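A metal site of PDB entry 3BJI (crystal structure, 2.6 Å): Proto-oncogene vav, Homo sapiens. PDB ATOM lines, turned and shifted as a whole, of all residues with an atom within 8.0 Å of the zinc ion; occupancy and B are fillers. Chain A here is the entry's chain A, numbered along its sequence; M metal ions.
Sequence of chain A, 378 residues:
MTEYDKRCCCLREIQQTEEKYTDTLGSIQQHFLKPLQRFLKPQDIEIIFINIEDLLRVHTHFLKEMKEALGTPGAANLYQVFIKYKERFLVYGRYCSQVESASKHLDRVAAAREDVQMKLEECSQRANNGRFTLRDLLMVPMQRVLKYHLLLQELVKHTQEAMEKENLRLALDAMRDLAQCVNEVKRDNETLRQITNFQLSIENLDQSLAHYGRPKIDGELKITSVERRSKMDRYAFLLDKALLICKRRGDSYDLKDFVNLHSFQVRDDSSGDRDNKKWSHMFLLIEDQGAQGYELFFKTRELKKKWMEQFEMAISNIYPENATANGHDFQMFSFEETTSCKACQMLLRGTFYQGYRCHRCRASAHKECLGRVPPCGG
A ring nitrogen (NE2) of His 366 lies within hydrogen-bond range of the backbone carbonyl oxygen (O) of Leu 347, at 2.5 Å.
N of Ala 343 sits close to SG of Cys 341 (3.6 Å).
The backbone NH (N) of Cys 341 lies within hydrogen-bond range of the backbone carbonyl oxygen (O) of Met 346, at 2.9 Å.
The side-chain sulfur of Cys 344 lies close to the backbone NH of Met 346 (3.6 Å).
The zinc ion is bound by SG of Cys 341 (2.1 Å), SG of Cys 369 (2.2 Å), ND1 of His 366 (2.2 Å) and SG of Cys 344 (2.3 Å).
The zinc ion has four donor atoms within binding distance.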
ATOM      1  N   SER A 340     -22.087  12.459   4.396  1.00  0.00           N
ATOM      2  CA  SER A 340     -21.607  13.844   4.505  1.00  0.00           C
ATOM      3  C   SER A 340     -20.426  14.236   3.569  1.00  0.00           C
ATOM      4  O   SER A 340     -19.709  13.388   3.010  1.00  0.00           O
ATOM      5  CB  SER A 340     -21.208  14.110   5.938  1.00  0.00           C
ATOM      6  OG  SER A 340     -20.428  13.041   6.421  1.00  0.00           O
ATOM      7  N   CYS A 341     -20.261  15.534   3.400  1.00  0.00           N
ATOM      8  CA  CYS A 341     -19.213  16.086   2.550  1.00  0.00           C
ATOM      9  C   CYS A 341     -17.853  16.083   3.245  1.00  0.00           C
ATOM     10  O   CYS A 341     -17.699  16.624   4.368  1.00  0.00           O
ATOM     11  CB  CYS A 341     -19.612  17.498   2.168  1.00  0.00           C
ATOM     12  SG  CYS A 341     -18.518  18.426   1.154  1.00  0.00           S
ATOM     13  N   LYS A 342     -16.852  15.515   2.589  1.00  0.00           N
ATOM     14  CA  LYS A 342     -15.509  15.417   3.169  1.00  0.00           C
ATOM     15  C   LYS A 342     -14.749  16.767   3.275  1.00  0.00           C
ATOM     16  O   LYS A 342     -13.704  16.826   3.925  1.00  0.00           O
ATOM     17  CB  LYS A 342     -14.670  14.385   2.409  1.00  0.00           C
ATOM     18  CG  LYS A 342     -13.633  13.666   3.286  1.00  0.00           C
ATOM     19  CD  LYS A 342     -12.708  12.732   2.449  1.00  0.00           C
ATOM     20  CE  LYS A 342     -11.426  12.292   3.193  1.00  0.00           C
ATOM     21  NZ  LYS A 342     -10.217  12.391   2.276  1.00  0.00           N
ATOM     22  N   ALA A 343     -15.258  17.839   2.664  1.00  0.00           N
ATOM     23  CA  ALA A 343     -14.708  19.177   2.851  1.00  0.00           C
ATOM     24  C   ALA A 343     -15.467  20.013   3.885  1.00  0.00           C
ATOM     25  O   ALA A 343     -14.836  20.631   4.734  1.00  0.00           O
ATOM     26  CB  ALA A 343     -14.693  19.921   1.555  1.00  0.00           C
ATOM     27  N   CYS A 344     -16.791  20.081   3.791  1.00  0.00           N
ATOM     28  CA  CYS A 344     -17.572  21.005   4.618  1.00  0.00           C
ATOM     29  C   CYS A 344     -18.214  20.294   5.797  1.00  0.00           C
ATOM     30  O   CYS A 344     -18.486  20.890   6.840  1.00  0.00           O
ATOM     31  CB  CYS A 344     -18.643  21.681   3.778  1.00  0.00           C
ATOM     32  SG  CYS A 344     -19.956  20.567   3.277  1.00  0.00           S
ATOM     33  N   GLN A 345     -18.510  19.016   5.592  1.00  0.00           N
ATOM     34  CA  GLN A 345     -18.988  18.126   6.650  1.00  0.00           C
ATOM     35  C   GLN A 345     -20.444  18.234   6.974  1.00  0.00           C
ATOM     36  O   GLN A 345     -20.935  17.504   7.816  1.00  0.00           O
ATOM     37  CB  GLN A 345     -18.149  18.271   7.913  1.00  0.00           C
ATOM     38  CG  GLN A 345     -18.069  16.940   8.675  1.00  0.00           C
ATOM     39  CD  GLN A 345     -16.709  16.709   9.290  1.00  0.00           C
ATOM     40  OE1 GLN A 345     -15.891  17.622   9.386  1.00  0.00           O
ATOM     41  NE2 GLN A 345     -16.470  15.475   9.720  1.00  0.00           N
ATOM     42  N   MET A 346     -21.166  19.110   6.282  1.00  0.00           N
ATOM     43  CA  MET A 346     -22.620  19.047   6.261  1.00  0.00           C
ATOM     44  C   MET A 346     -23.048  17.821   5.428  1.00  0.00           C
ATOM     45  O   MET A 346     -22.210  17.097   4.898  1.00  0.00           O
ATOM     46  CB  MET A 346     -23.205  20.356   5.735  1.00  0.00           C
ATOM     47  CG  MET A 346     -22.894  21.591   6.641  1.00  0.00           C
ATOM     48  SD  MET A 346     -23.228  21.391   8.426  1.00  0.00           S
ATOM     49  CE  MET A 346     -21.798  20.529   9.005  1.00  0.00           C
ATOM     50  N   LEU A 347     -24.355  17.561   5.332  1.00  0.00           N
ATOM     51  CA  LEU A 347     -24.809  16.371   4.644  1.00  0.00           C
ATOM     52  C   LEU A 347     -24.929  16.632   3.147  1.00  0.00           C
ATOM     53  O   LEU A 347     -25.166  17.773   2.700  1.00  0.00           O
ATOM     54  CB  LEU A 347     -26.165  15.907   5.194  1.00  0.00           C
ATOM     55  CG  LEU A 347     -26.270  15.254   6.593  1.00  0.00           C
ATOM     56  CD1 LEU A 347     -27.651  15.553   7.212  1.00  0.00           C
ATOM     57  CD2 LEU A 347     -25.995  13.737   6.595  1.00  0.00           C
ATOM     58  N   LEU A 348     -24.741  15.558   2.381  1.00  0.00           N
ATOM     59  CA  LEU A 348     -25.217  15.528   1.033  1.00  0.00           C
ATOM     60  C   LEU A 348     -26.707  15.381   1.172  1.00  0.00           C
ATOM     61  O   LEU A 348     -27.174  14.547   1.922  1.00  0.00           O
ATOM     62  CB  LEU A 348     -24.612  14.357   0.239  1.00  0.00           C
ATOM     63  CG  LEU A 348     -23.250  14.665  -0.400  1.00  0.00           C
ATOM     64  CD1 LEU A 348     -22.221  15.210   0.594  1.00  0.00           C
ATOM     65  CD2 LEU A 348     -22.707  13.430  -1.051  1.00  0.00           C
ATOM     66  N   ARG A 349     -27.441  16.204   0.442  1.00  0.00           N
ATOM     67  CA  ARG A 349     -28.857  16.374   0.663  1.00  0.00           C
ATOM     68  C   ARG A 349     -29.677  15.659  -0.413  1.00  0.00           C
ATOM     69  O   ARG A 349     -29.463  15.879  -1.615  1.00  0.00           O
ATOM     70  CB  ARG A 349     -29.206  17.853   0.589  1.00  0.00           C
ATOM     71  CG  ARG A 349     -28.216  18.811   1.252  1.00  0.00           C
ATOM     72  CD  ARG A 349     -28.768  19.483   2.457  1.00  0.00           C
ATOM     73  NE  ARG A 349     -27.797  20.250   3.270  1.00  0.00           N
ATOM     74  CZ  ARG A 349     -26.709  20.899   2.832  1.00  0.00           C
ATOM     75  NH1 ARG A 349     -26.358  20.962   1.564  1.00  0.00           N
ATOM     76  NH2 ARG A 349     -25.939  21.530   3.719  1.00  0.00           N
ATOM     77  N   SER A 364     -16.744  11.636  -0.687  1.00  0.00           N
ATOM     78  CA  SER A 364     -18.054  12.193  -1.000  1.00  0.00           C
ATOM     79  C   SER A 364     -18.078  13.685  -0.847  1.00  0.00           C
ATOM     80  O   SER A 364     -17.555  14.198   0.137  1.00  0.00           O
ATOM     81  CB  SER A 364     -19.080  11.627  -0.047  1.00  0.00           C
ATOM     82  OG  SER A 364     -19.082  10.215  -0.074  1.00  0.00           O
ATOM     83  N   ALA A 365     -18.747  14.400  -1.760  1.00  0.00           N
ATOM     84  CA  ALA A 365     -18.690  15.846  -1.718  1.00  0.00           C
ATOM     85  C   ALA A 365     -19.809  16.549  -2.482  1.00  0.00           C
ATOM     86  O   ALA A 365     -20.324  16.009  -3.473  1.00  0.00           O
ATOM     87  CB  ALA A 365     -17.354  16.293  -2.254  1.00  0.00           C
ATOM     88  N   HIS A 366     -20.192  17.744  -2.025  1.00  0.00           N
ATOM     89  CA  HIS A 366     -21.130  18.558  -2.789  1.00  0.00           C
ATOM     90  C   HIS A 366     -20.445  19.098  -4.078  1.00  0.00           C
ATOM     91  O   HIS A 366     -19.228  19.242  -4.120  1.00  0.00           O
ATOM     92  CB  HIS A 366     -21.655  19.742  -1.962  1.00  0.00           C
ATOM     93  CG  HIS A 366     -22.252  19.367  -0.635  1.00  0.00           C
ATOM     94  ND1 HIS A 366     -21.505  19.252   0.519  1.00  0.00           N
ATOM     95  CD2 HIS A 366     -23.538  19.146  -0.267  1.00  0.00           C
ATOM     96  CE1 HIS A 366     -22.294  18.926   1.526  1.00  0.00           C
ATOM     97  NE2 HIS A 366     -23.534  18.865   1.076  1.00  0.00           N
ATOM     98  N   LYS A 367     -21.214  19.441  -5.113  1.00  0.00           N
ATOM     99  CA  LYS A 367     -20.629  20.038  -6.321  1.00  0.00           C
ATOM    100  C   LYS A 367     -19.717  21.221  -5.977  1.00  0.00           C
ATOM    101  O   LYS A 367     -18.631  21.363  -6.537  1.00  0.00           O
ATOM    102  CB  LYS A 367     -21.721  20.497  -7.303  1.00  0.00           C
ATOM    103  CG  LYS A 367     -21.177  21.347  -8.397  1.00  0.00           C
ATOM    104  CD  LYS A 367     -21.504  20.886  -9.818  1.00  0.00           C
ATOM    105  CE  LYS A 367     -22.687  21.581 -10.454  1.00  0.00           C
ATOM    106  NZ  LYS A 367     -22.480  21.642 -11.915  1.00  0.00           N
ATOM    107  N   GLU A 368     -20.164  22.048  -5.040  1.00  0.00           N
ATOM    108  CA  GLU A 368     -19.522  23.307  -4.721  1.00  0.00           C
ATOM    109  C   GLU A 368     -18.319  23.126  -3.813  1.00  0.00           C
ATOM    110  O   GLU A 368     -17.656  24.105  -3.503  1.00  0.00           O
ATOM    111  CB  GLU A 368     -20.500  24.287  -4.023  1.00  0.00           C
ATOM    112  CG  GLU A 368     -21.981  24.067  -4.272  1.00  0.00           C
ATOM    113  CD  GLU A 368     -22.592  23.003  -3.354  1.00  0.00           C
ATOM    114  OE1 GLU A 368     -23.040  21.941  -3.866  1.00  0.00           O
ATOM    115  OE2 GLU A 368     -22.618  23.241  -2.110  1.00  0.00           O
ATOM    116  N   CYS A 369     -18.064  21.895  -3.349  1.00  0.00           N
ATOM    117  CA  CYS A 369     -17.006  21.636  -2.353  1.00  0.00           C
ATOM    118  C   CYS A 369     -15.792  20.822  -2.893  1.00  0.00           C
ATOM    119  O   CYS A 369     -14.926  20.420  -2.128  1.00  0.00           O
ATOM    120  CB  CYS A 369     -17.642  20.929  -1.130  1.00  0.00           C
ATOM    121  SG  CYS A 369     -18.850  21.949  -0.087  1.00  0.00           S
ATOM    122  N   LEU A 370     -15.728  20.600  -4.213  1.00  0.00           N
ATOM    123  CA  LEU A 370     -14.779  19.635  -4.805  1.00  0.00           C
ATOM    124  C   LEU A 370     -13.314  20.066  -4.703  1.00  0.00           C
ATOM    125  O   LEU A 370     -12.444  19.299  -4.289  1.00  0.00           O
ATOM    126  CB  LEU A 370     -15.136  19.366  -6.265  1.00  0.00           C
ATOM    127  CG  LEU A 370     -16.509  18.763  -6.587  1.00  0.00           C
ATOM    128  CD1 LEU A 370     -16.592  18.385  -8.042  1.00  0.00           C
ATOM    129  CD2 LEU A 370     -16.850  17.554  -5.727  1.00  0.00           C
ATOM    130  N   ARG A 372     -12.166  21.737  -2.488  1.00  0.00           N
ATOM    131  CA  ARG A 372     -11.791  21.907  -1.087  1.00  0.00           C
ATOM    132  C   ARG A 372     -11.575  20.579  -0.394  1.00  0.00           C
ATOM    133  O   ARG A 372     -11.199  20.541   0.767  1.00  0.00           O
ATOM    134  CB  ARG A 372     -12.842  22.721  -0.383  1.00  0.00           C
ATOM    135  CG  ARG A 372     -12.299  23.484   0.794  1.00  0.00           C
ATOM    136  CD  ARG A 372     -13.158  24.706   1.032  1.00  0.00           C
ATOM    137  NE  ARG A 372     -13.036  25.670  -0.072  1.00  0.00           N
ATOM    138  CZ  ARG A 372     -14.015  26.452  -0.514  1.00  0.00           C
ATOM    139  NH1 ARG A 372     -15.255  26.370   0.006  1.00  0.00           N
ATOM    140  NH2 ARG A 372     -13.784  27.312  -1.512  1.00  0.00           N
ATOM    141  N   VAL A 373     -11.782  19.476  -1.093  1.00  0.00           N
ATOM    142  CA  VAL A 373     -11.568  18.173  -0.466  1.00  0.00           C
ATOM    143  C   VAL A 373     -10.075  17.865  -0.270  1.00  0.00           C
ATOM    144  O   VAL A 373      -9.260  18.043  -1.182  1.00  0.00           O
ATOM    145  CB  VAL A 373     -12.271  17.048  -1.255  1.00  0.00           C
ATOM    146  CG1 VAL A 373     -12.104  15.716  -0.568  1.00  0.00           C
ATOM    147  CG2 VAL A 373     -13.726  17.400  -1.434  1.00  0.00           C
HETATM  148 ZN    ZN M   1     -19.610  20.263   1.070  1.00  0.00          ZN
